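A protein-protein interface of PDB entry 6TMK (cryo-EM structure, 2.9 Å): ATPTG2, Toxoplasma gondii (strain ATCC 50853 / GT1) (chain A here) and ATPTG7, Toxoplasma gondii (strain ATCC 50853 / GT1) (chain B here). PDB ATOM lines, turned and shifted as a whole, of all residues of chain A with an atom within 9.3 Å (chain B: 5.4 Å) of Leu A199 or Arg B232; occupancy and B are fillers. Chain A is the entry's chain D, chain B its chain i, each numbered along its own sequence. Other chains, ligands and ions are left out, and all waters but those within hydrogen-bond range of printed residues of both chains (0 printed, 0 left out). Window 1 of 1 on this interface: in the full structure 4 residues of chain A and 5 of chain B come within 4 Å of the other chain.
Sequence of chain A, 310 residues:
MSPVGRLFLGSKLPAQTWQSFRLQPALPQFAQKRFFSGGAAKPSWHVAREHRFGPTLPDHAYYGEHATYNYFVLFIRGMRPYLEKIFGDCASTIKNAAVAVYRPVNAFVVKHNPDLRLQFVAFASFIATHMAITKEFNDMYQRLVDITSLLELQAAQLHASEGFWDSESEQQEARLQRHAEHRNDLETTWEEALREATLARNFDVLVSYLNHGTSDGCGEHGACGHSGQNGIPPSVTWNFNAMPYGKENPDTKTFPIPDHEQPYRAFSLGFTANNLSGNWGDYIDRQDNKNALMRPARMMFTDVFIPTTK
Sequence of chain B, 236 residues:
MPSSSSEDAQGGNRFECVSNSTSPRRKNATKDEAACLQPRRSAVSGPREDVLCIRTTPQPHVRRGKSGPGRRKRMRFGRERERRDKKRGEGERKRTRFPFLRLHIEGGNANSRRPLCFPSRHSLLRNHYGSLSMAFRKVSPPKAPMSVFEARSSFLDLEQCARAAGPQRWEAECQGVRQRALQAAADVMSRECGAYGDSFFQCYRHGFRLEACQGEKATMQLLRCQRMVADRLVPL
Among the printed residues, pairs that only touch across the chains: Arg A195 with Tyr B196 (3.6 Å) and Leu A199 with Met B228 (3.8 Å).
NE of Arg A201 lies close to NE of Arg B232.
OE2 of Glu A196 lies within salt-bridge range of NH1 of Arg B224, at 3.2 Å.
NH2 of Arg A201 is in salt-bridge range of OE1 of Glu B192.
NH2 of Arg B232 sits at hydrogen-bond distance from O of Leu A199, at 3.3 Å.
Arg B232 touches just these residues of chain A: Leu A199 and Arg A201.
Of the printed residues of chain A, Glu B192 touches Arg A201.
Of the printed residues of chain B, Arg A195 touches Tyr B196.
Glu A191 touches none of the printed residues of chain B.
Leu A194 touches none of the printed residues of chain B.
The nearest residue of chain B that does not touch Leu A199 is Tyr B196 (4.1 Å).
The nearest printed residue of chain B that does not touch Arg A201 is Val B148 (5.8 Å).
The side-chain carboxylate of Glu B192 is in salt-bridge range of the guanidinium group of Arg B232 (2.7 Å).
Printed residues of chain A that touch a printed residue of chain B: Arg A195, Glu A196, Leu A199 and Arg A201.
Of the 15 printed residues of chain B, 5 touch a printed residue of chain A.
Printed residues of chain B that touch a printed residue of chain A: Glu B192, Tyr B196, Arg B224, Met B228 and Arg B232.
Among the printed residues, 6 pairs touch across the chains.
Among the printed residues, Asp or Glu carboxylates within 4 Å of a Lys or Arg side-chain nitrogen of the other chain: Glu A196 with Arg B224 (3.2 Å) and Arg A201 with Glu B192 (3.5 Å).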
ATOM      1  N   GLU A 191     -19.806  24.557 -15.193  1.00  0.00           N
ATOM      2  CA  GLU A 191     -20.469  23.417 -14.571  1.00  0.00           C
ATOM      3  C   GLU A 191     -19.733  22.121 -14.888  1.00  0.00           C
ATOM      4  O   GLU A 191     -19.452  21.313 -13.991  1.00  0.00           O
ATOM      5  CB  GLU A 191     -21.915  23.347 -15.045  1.00  0.00           C
ATOM      6  CG  GLU A 191     -22.771  24.466 -14.534  1.00  0.00           C
ATOM      7  CD  GLU A 191     -24.108  24.540 -15.240  1.00  0.00           C
ATOM      8  OE1 GLU A 191     -24.379  23.670 -16.093  1.00  0.00           O
ATOM      9  OE2 GLU A 191     -24.890  25.470 -14.948  1.00  0.00           O
ATOM     10  N   GLU A 192     -19.395  21.915 -16.161  1.00  0.00           N
ATOM     11  CA  GLU A 192     -18.666  20.712 -16.545  1.00  0.00           C
ATOM     12  C   GLU A 192     -17.318  20.626 -15.835  1.00  0.00           C
ATOM     13  O   GLU A 192     -16.941  19.566 -15.311  1.00  0.00           O
ATOM     14  CB  GLU A 192     -18.477  20.692 -18.056  1.00  0.00           C
ATOM     15  CG  GLU A 192     -18.029  19.372 -18.614  1.00  0.00           C
ATOM     16  CD  GLU A 192     -17.893  19.410 -20.115  1.00  0.00           C
ATOM     17  OE1 GLU A 192     -17.935  20.523 -20.680  1.00  0.00           O
ATOM     18  OE2 GLU A 192     -17.750  18.333 -20.730  1.00  0.00           O
ATOM     19  N   ALA A 193     -16.573  21.731 -15.820  1.00  0.00           N
ATOM     20  CA  ALA A 193     -15.259  21.739 -15.197  1.00  0.00           C
ATOM     21  C   ALA A 193     -15.346  21.431 -13.715  1.00  0.00           C
ATOM     22  O   ALA A 193     -14.537  20.664 -13.185  1.00  0.00           O
ATOM     23  CB  ALA A 193     -14.594  23.094 -15.417  1.00  0.00           C
ATOM     24  N   LEU A 194     -16.311  22.031 -13.024  1.00  0.00           N
ATOM     25  CA  LEU A 194     -16.445  21.790 -11.596  1.00  0.00           C
ATOM     26  C   LEU A 194     -16.828  20.348 -11.316  1.00  0.00           C
ATOM     27  O   LEU A 194     -16.321  19.741 -10.370  1.00  0.00           O
ATOM     28  CB  LEU A 194     -17.468  22.744 -10.998  1.00  0.00           C
ATOM     29  CG  LEU A 194     -17.569  22.704  -9.480  1.00  0.00           C
ATOM     30  CD1 LEU A 194     -16.296  23.204  -8.839  1.00  0.00           C
ATOM     31  CD2 LEU A 194     -18.742  23.509  -9.023  1.00  0.00           C
ATOM     32  N   ARG A 195     -17.698  19.766 -12.141  1.00  0.00           N
ATOM     33  CA  ARG A 195     -18.065  18.369 -11.942  1.00  0.00           C
ATOM     34  C   ARG A 195     -16.853  17.458 -12.097  1.00  0.00           C
ATOM     35  O   ARG A 195     -16.596  16.587 -11.252  1.00  0.00           O
ATOM     36  CB  ARG A 195     -19.166  17.978 -12.921  1.00  0.00           C
ATOM     37  CG  ARG A 195     -20.535  18.387 -12.463  1.00  0.00           C
ATOM     38  CD  ARG A 195     -21.623  17.737 -13.275  1.00  0.00           C
ATOM     39  NE  ARG A 195     -22.076  18.573 -14.381  1.00  0.00           N
ATOM     40  CZ  ARG A 195     -21.707  18.418 -15.647  1.00  0.00           C
ATOM     41  NH1 ARG A 195     -20.868  17.460 -15.998  1.00  0.00           N
ATOM     42  NH2 ARG A 195     -22.181  19.231 -16.569  1.00  0.00           N
ATOM     43  N   GLU A 196     -16.100  17.640 -13.180  1.00  0.00           N
ATOM     44  CA  GLU A 196     -14.948  16.785 -13.428  1.00  0.00           C
ATOM     45  C   GLU A 196     -13.871  16.974 -12.367  1.00  0.00           C
ATOM     46  O   GLU A 196     -13.289  15.995 -11.883  1.00  0.00           O
ATOM     47  CB  GLU A 196     -14.393  17.069 -14.816  1.00  0.00           C
ATOM     48  CG  GLU A 196     -15.316  16.634 -15.930  1.00  0.00           C
ATOM     49  CD  GLU A 196     -15.171  15.165 -16.285  1.00  0.00           C
ATOM     50  OE1 GLU A 196     -14.103  14.581 -16.007  1.00  0.00           O
ATOM     51  OE2 GLU A 196     -16.129  14.595 -16.849  1.00  0.00           O
ATOM     52  N   ALA A 197     -13.612  18.218 -11.970  1.00  0.00           N
ATOM     53  CA  ALA A 197     -12.616  18.475 -10.945  1.00  0.00           C
ATOM     54  C   ALA A 197     -13.068  18.013  -9.572  1.00  0.00           C
ATOM     55  O   ALA A 197     -12.223  17.749  -8.719  1.00  0.00           O
ATOM     56  CB  ALA A 197     -12.288  19.962 -10.897  1.00  0.00           C
ATOM     57  N   THR A 198     -14.373  17.903  -9.340  1.00  0.00           N
ATOM     58  CA  THR A 198     -14.850  17.383  -8.070  1.00  0.00           C
ATOM     59  C   THR A 198     -14.728  15.870  -8.014  1.00  0.00           C
ATOM     60  O   THR A 198     -14.356  15.314  -6.975  1.00  0.00           O
ATOM     61  CB  THR A 198     -16.298  17.804  -7.837  1.00  0.00           C
ATOM     62  OG1 THR A 198     -16.362  19.219  -7.636  1.00  0.00           O
ATOM     63  CG2 THR A 198     -16.867  17.096  -6.628  1.00  0.00           C
ATOM     64  N   LEU A 199     -15.032  15.181  -9.115  1.00  0.00           N
ATOM     65  CA  LEU A 199     -14.887  13.730  -9.083  1.00  0.00           C
ATOM     66  C   LEU A 199     -13.422  13.318  -9.103  1.00  0.00           C
ATOM     67  O   LEU A 199     -13.071  12.271  -8.548  1.00  0.00           O
ATOM     68  CB  LEU A 199     -15.638  13.072 -10.242  1.00  0.00           C
ATOM     69  CG  LEU A 199     -15.169  13.321 -11.671  1.00  0.00           C
ATOM     70  CD1 LEU A 199     -14.061  12.362 -12.051  1.00  0.00           C
ATOM     71  CD2 LEU A 199     -16.324  13.154 -12.622  1.00  0.00           C
ATOM     72  N   ALA A 200     -12.556  14.114  -9.727  1.00  0.00           N
ATOM     73  CA  ALA A 200     -11.129  13.827  -9.730  1.00  0.00           C
ATOM     74  C   ALA A 200     -10.407  14.362  -8.502  1.00  0.00           C
ATOM     75  O   ALA A 200      -9.328  13.859  -8.168  1.00  0.00           O
ATOM     76  CB  ALA A 200     -10.475  14.412 -10.980  1.00  0.00           C
ATOM     77  N   ARG A 201     -10.972  15.357  -7.827  1.00  0.00           N
ATOM     78  CA  ARG A 201     -10.318  16.055  -6.728  1.00  0.00           C
ATOM     79  C   ARG A 201      -8.937  16.554  -7.151  1.00  0.00           C
ATOM     80  O   ARG A 201      -7.899  16.144  -6.631  1.00  0.00           O
ATOM     81  CB  ARG A 201     -10.252  15.159  -5.497  1.00  0.00           C
ATOM     82  CG  ARG A 201     -11.556  15.177  -4.735  1.00  0.00           C
ATOM     83  CD  ARG A 201     -11.752  13.959  -3.870  1.00  0.00           C
ATOM     84  NE  ARG A 201     -13.161  13.586  -3.827  1.00  0.00           N
ATOM     85  CZ  ARG A 201     -14.097  14.295  -3.208  1.00  0.00           C
ATOM     86  NH1 ARG A 201     -13.776  15.411  -2.574  1.00  0.00           N
ATOM     87  NH2 ARG A 201     -15.357  13.887  -3.219  1.00  0.00           N
ATOM     88  N   ASN A 202      -8.956  17.468  -8.120  1.00  0.00           N
ATOM     89  CA  ASN A 202      -7.732  18.032  -8.669  1.00  0.00           C
ATOM     90  C   ASN A 202      -8.033  19.402  -9.261  1.00  0.00           C
ATOM     91  O   ASN A 202      -8.995  19.559 -10.016  1.00  0.00           O
ATOM     92  CB  ASN A 202      -7.141  17.106  -9.731  1.00  0.00           C
ATOM     93  CG  ASN A 202      -5.700  17.424 -10.043  1.00  0.00           C
ATOM     94  OD1 ASN A 202      -5.036  18.150  -9.306  1.00  0.00           O
ATOM     95  ND2 ASN A 202      -5.205  16.876 -11.140  1.00  0.00           N
ATOM     96  N   VAL A 205      -7.384  20.192 -13.229  1.00  0.00           N
ATOM     97  CA  VAL A 205      -8.469  19.942 -14.173  1.00  0.00           C
ATOM     98  C   VAL A 205      -9.243  21.228 -14.449  1.00  0.00           C
ATOM     99  O   VAL A 205      -9.502  21.589 -15.605  1.00  0.00           O
ATOM    100  CB  VAL A 205      -9.381  18.829 -13.637  1.00  0.00           C
ATOM    101  CG1 VAL A 205     -10.543  18.605 -14.558  1.00  0.00           C
ATOM    102  CG2 VAL A 205      -8.595  17.553 -13.471  1.00  0.00           C
ATOM    103  N   TYR A 209      -9.587  23.306 -18.051  1.00  0.00           N
ATOM    104  CA  TYR A 209     -10.803  23.760 -18.718  1.00  0.00           C
ATOM    105  C   TYR A 209     -10.773  25.236 -19.092  1.00  0.00           C
ATOM    106  O   TYR A 209     -11.759  25.730 -19.648  1.00  0.00           O
ATOM    107  CB  TYR A 209     -12.036  23.455 -17.869  1.00  0.00           C
ATOM    108  CG  TYR A 209     -12.435  22.001 -17.877  1.00  0.00           C
ATOM    109  CD1 TYR A 209     -13.134  21.482 -18.950  1.00  0.00           C
ATOM    110  CD2 TYR A 209     -12.098  21.146 -16.846  1.00  0.00           C
ATOM    111  CE1 TYR A 209     -13.508  20.168 -18.990  1.00  0.00           C
ATOM    112  CE2 TYR A 209     -12.468  19.822 -16.881  1.00  0.00           C
ATOM    113  CZ  TYR A 209     -13.164  19.337 -17.962  1.00  0.00           C
ATOM    114  OH  TYR A 209     -13.539  18.018 -18.014  1.00  0.00           O
ATOM    115  N   VAL B 148     -18.174   9.991   3.893  1.00  0.00           N
ATOM    116  CA  VAL B 148     -16.991   9.278   3.427  1.00  0.00           C
ATOM    117  C   VAL B 148     -16.154   8.801   4.604  1.00  0.00           C
ATOM    118  O   VAL B 148     -15.626   7.684   4.600  1.00  0.00           O
ATOM    119  CB  VAL B 148     -16.174  10.178   2.484  1.00  0.00           C
ATOM    120  CG1 VAL B 148     -14.889   9.503   2.095  1.00  0.00           C
ATOM    121  CG2 VAL B 148     -16.976  10.523   1.258  1.00  0.00           C
ATOM    122  N   ARG B 152     -15.366   4.879   5.320  1.00  0.00           N
ATOM    123  CA  ARG B 152     -13.987   4.425   5.411  1.00  0.00           C
ATOM    124  C   ARG B 152     -13.726   3.718   6.735  1.00  0.00           C
ATOM    125  O   ARG B 152     -13.077   2.663   6.773  1.00  0.00           O
ATOM    126  CB  ARG B 152     -13.068   5.625   5.222  1.00  0.00           C
ATOM    127  CG  ARG B 152     -11.611   5.309   5.054  1.00  0.00           C
ATOM    128  CD  ARG B 152     -10.874   6.590   4.743  1.00  0.00           C
ATOM    129  NE  ARG B 152     -11.240   7.094   3.423  1.00  0.00           N
ATOM    130  CZ  ARG B 152     -10.917   8.298   2.968  1.00  0.00           C
ATOM    131  NH1 ARG B 152     -10.220   9.133   3.724  1.00  0.00           N
ATOM    132  NH2 ARG B 152     -11.294   8.669   1.754  1.00  0.00           N
ATOM    133  N   VAL B 188     -22.802   7.049  -0.203  1.00  0.00           N
ATOM    134  CA  VAL B 188     -21.809   7.924  -0.819  1.00  0.00           C
ATOM    135  C   VAL B 188     -21.969   7.922  -2.334  1.00  0.00           C
ATOM    136  O   VAL B 188     -21.928   8.974  -2.985  1.00  0.00           O
ATOM    137  CB  VAL B 188     -20.392   7.493  -0.408  1.00  0.00           C
ATOM    138  CG1 VAL B 188     -19.364   8.234  -1.215  1.00  0.00           C
ATOM    139  CG2 VAL B 188     -20.184   7.729   1.056  1.00  0.00           C
ATOM    140  N   GLU B 192     -22.869  11.194  -4.659  1.00  0.00           N
ATOM    141  CA  GLU B 192     -21.881  11.731  -5.584  1.00  0.00           C
ATOM    142  C   GLU B 192     -22.151  11.409  -7.048  1.00  0.00           C
ATOM    143  O   GLU B 192     -21.522  12.016  -7.920  1.00  0.00           O
ATOM    144  CB  GLU B 192     -20.489  11.216  -5.214  1.00  0.00           C
ATOM    145  CG  GLU B 192     -20.007  11.665  -3.853  1.00  0.00           C
ATOM    146  CD  GLU B 192     -18.547  11.342  -3.614  1.00  0.00           C
ATOM    147  OE1 GLU B 192     -18.031  11.682  -2.529  1.00  0.00           O
ATOM    148  OE2 GLU B 192     -17.914  10.751  -4.512  1.00  0.00           O
ATOM    149  N   TYR B 196     -25.759  12.038 -12.481  1.00  0.00           N
ATOM    150  CA  TYR B 196     -25.522  11.281 -13.702  1.00  0.00           C
ATOM    151  C   TYR B 196     -26.552  10.174 -13.877  1.00  0.00           C
ATOM    152  O   TYR B 196     -26.990   9.895 -15.000  1.00  0.00           O
ATOM    153  CB  TYR B 196     -24.116  10.696 -13.672  1.00  0.00           C
ATOM    154  CG  TYR B 196     -23.021  11.730 -13.654  1.00  0.00           C
ATOM    155  CD1 TYR B 196     -22.858  12.620 -14.699  1.00  0.00           C
ATOM    156  CD2 TYR B 196     -22.152  11.817 -12.581  1.00  0.00           C
ATOM    157  CE1 TYR B 196     -21.858  13.563 -14.678  1.00  0.00           C
ATOM    158  CE2 TYR B 196     -21.153  12.755 -12.554  1.00  0.00           C
ATOM    159  CZ  TYR B 196     -21.008  13.625 -13.603  1.00  0.00           C
ATOM    160  OH  TYR B 196     -20.006  14.560 -13.565  1.00  0.00           O
ATOM    161  N   ARG B 224     -17.691   6.170 -14.569  1.00  0.00           N
ATOM    162  CA  ARG B 224     -16.480   6.783 -14.042  1.00  0.00           C
ATOM    163  C   ARG B 224     -16.690   7.280 -12.619  1.00  0.00           C
ATOM    164  O   ARG B 224     -15.808   7.129 -11.767  1.00  0.00           O
ATOM    165  CB  ARG B 224     -16.047   7.919 -14.958  1.00  0.00           C
ATOM    166  CG  ARG B 224     -14.622   8.381 -14.760  1.00  0.00           C
ATOM    167  CD  ARG B 224     -14.364   9.653 -15.536  1.00  0.00           C
ATOM    168  NE  ARG B 224     -14.694   9.477 -16.948  1.00  0.00           N
ATOM    169  CZ  ARG B 224     -15.427  10.321 -17.669  1.00  0.00           C
ATOM    170  NH1 ARG B 224     -15.921  11.428 -17.134  1.00  0.00           N
ATOM    171  NH2 ARG B 224     -15.668  10.054 -18.942  1.00  0.00           N
ATOM    172  N   ARG B 227     -16.589   4.192 -10.414  1.00  0.00           N
ATOM    173  CA  ARG B 227     -15.227   3.696 -10.274  1.00  0.00           C
ATOM    174  C   ARG B 227     -14.420   4.576  -9.328  1.00  0.00           C
ATOM    175  O   ARG B 227     -13.667   4.071  -8.487  1.00  0.00           O
ATOM    176  CB  ARG B 227     -14.563   3.628 -11.646  1.00  0.00           C
ATOM    177  CG  ARG B 227     -13.183   3.003 -11.654  1.00  0.00           C
ATOM    178  CD  ARG B 227     -13.252   1.502 -11.499  1.00  0.00           C
ATOM    179  NE  ARG B 227     -13.599   0.852 -12.758  1.00  0.00           N
ATOM    180  CZ  ARG B 227     -12.755   0.684 -13.770  1.00  0.00           C
ATOM    181  NH1 ARG B 227     -11.507   1.124 -13.685  1.00  0.00           N
ATOM    182  NH2 ARG B 227     -13.162   0.081 -14.876  1.00  0.00           N
ATOM    183  N   MET B 228     -14.562   5.896  -9.454  1.00  0.00           N
ATOM    184  CA  MET B 228     -13.824   6.807  -8.589  1.00  0.00           C
ATOM    185  C   MET B 228     -14.249   6.643  -7.137  1.00  0.00           C
ATOM    186  O   MET B 228     -13.408   6.629  -6.233  1.00  0.00           O
ATOM    187  CB  MET B 228     -14.041   8.246  -9.043  1.00  0.00           C
ATOM    188  CG  MET B 228     -13.420   8.580 -10.385  1.00  0.00           C
ATOM    189  SD  MET B 228     -11.695   9.076 -10.249  1.00  0.00           S
ATOM    190  CE  MET B 228     -11.396   9.702 -11.899  1.00  0.00           C
ATOM    191  N   VAL B 229     -15.553   6.509  -6.896  1.00  0.00           N
ATOM    192  CA  VAL B 229     -16.036   6.330  -5.531  1.00  0.00           C
ATOM    193  C   VAL B 229     -15.468   5.052  -4.930  1.00  0.00           C
ATOM    194  O   VAL B 229     -15.001   5.035  -3.784  1.00  0.00           O
ATOM    195  CB  VAL B 229     -17.573   6.327  -5.505  1.00  0.00           C
ATOM    196  CG1 VAL B 229     -18.071   5.833  -4.170  1.00  0.00           C
ATOM    197  CG2 VAL B 229     -18.095   7.712  -5.782  1.00  0.00           C
ATOM    198  N   ALA B 230     -15.503   3.959  -5.690  1.00  0.00           N
ATOM    199  CA  ALA B 230     -14.964   2.703  -5.183  1.00  0.00           C
ATOM    200  C   ALA B 230     -13.476   2.829  -4.878  1.00  0.00           C
ATOM    201  O   ALA B 230     -13.019   2.462  -3.787  1.00  0.00           O
ATOM    202  CB  ALA B 230     -15.214   1.586  -6.194  1.00  0.00           C
ATOM    203  N   ASP B 231     -12.704   3.356  -5.830  1.00  0.00           N
ATOM    204  CA  ASP B 231     -11.270   3.522  -5.628  1.00  0.00           C
ATOM    205  C   ASP B 231     -10.964   4.422  -4.440  1.00  0.00           C
ATOM    206  O   ASP B 231      -9.916   4.276  -3.802  1.00  0.00           O
ATOM    207  CB  ASP B 231     -10.633   4.088  -6.894  1.00  0.00           C
ATOM    208  CG  ASP B 231     -10.699   3.124  -8.059  1.00  0.00           C
ATOM    209  OD1 ASP B 231     -11.115   1.964  -7.850  1.00  0.00           O
ATOM    210  OD2 ASP B 231     -10.334   3.522  -9.185  1.00  0.00           O
ATOM    211  N   ARG B 232     -11.856   5.360  -4.134  1.00  0.00           N
ATOM    212  CA  ARG B 232     -11.663   6.227  -2.979  1.00  0.00           C
ATOM    213  C   ARG B 232     -12.015   5.530  -1.675  1.00  0.00           C
ATOM    214  O   ARG B 232     -11.424   5.838  -0.634  1.00  0.00           O
ATOM    215  CB  ARG B 232     -12.505   7.490  -3.131  1.00  0.00           C
ATOM    216  CG  ARG B 232     -11.947   8.695  -2.413  1.00  0.00           C
ATOM    217  CD  ARG B 232     -12.874   9.885  -2.548  1.00  0.00           C
ATOM    218  NE  ARG B 232     -13.054  10.273  -3.945  1.00  0.00           N
ATOM    219  CZ  ARG B 232     -14.228  10.522  -4.522  1.00  0.00           C
ATOM    220  NH1 ARG B 232     -15.356  10.446  -3.832  1.00  0.00           N
ATOM    221  NH2 ARG B 232     -14.269  10.866  -5.800  1.00  0.00           N
ATOM    222  N   LEU B 233     -12.969   4.603  -1.706  1.00  0.00           N
ATOM    223  CA  LEU B 233     -13.462   3.985  -0.479  1.00  0.00           C
ATOM    224  C   LEU B 233     -12.695   2.722  -0.098  1.00  0.00           C
ATOM    225  O   LEU B 233     -12.090   2.661   0.976  1.00  0.00           O
ATOM    226  CB  LEU B 233     -14.948   3.657  -0.625  1.00  0.00           C
ATOM    227  CG  LEU B 233     -15.893   4.847  -0.736  1.00  0.00           C
ATOM    228  CD1 LEU B 233     -17.292   4.363  -1.030  1.00  0.00           C
ATOM    229  CD2 LEU B 233     -15.868   5.664   0.529  1.00  0.00           C
ATOM    230  N   VAL B 234     -12.711   1.708  -0.957  1.00  0.00           N
ATOM    231  CA  VAL B 234     -12.334   0.364  -0.521  1.00  0.00           C
ATOM    232  C   VAL B 234     -10.832   0.239  -0.280  1.00  0.00           C
ATOM    233  O   VAL B 234     -10.434  -0.436   0.680  1.00  0.00           O
ATOM    234  CB  VAL B 234     -12.816  -0.705  -1.518  1.00  0.00           C
ATOM    235  CG1 VAL B 234     -12.137  -0.567  -2.868  1.00  0.00           C
ATOM    236  CG2 VAL B 234     -12.581  -2.089  -0.948  1.00  0.00           C
ATOM    237  N   PRO B 235      -9.953   0.848  -1.092  1.00  0.00           N
ATOM    238  CA  PRO B 235      -8.544   0.574  -0.789  1.00  0.00           C
ATOM    239  C   PRO B 235      -8.055   1.305   0.459  1.00  0.00           C
ATOM    240  O   PRO B 235      -8.178   0.759   1.557  1.00  0.00           O
ATOM    241  CB  PRO B 235      -7.807   1.079  -2.042  1.00  0.00           C
ATOM    242  CG  PRO B 235      -8.887   1.480  -3.027  1.00  0.00           C
ATOM    243  CD  PRO B 235     -10.075   1.813  -2.191  1.00  0.00           C
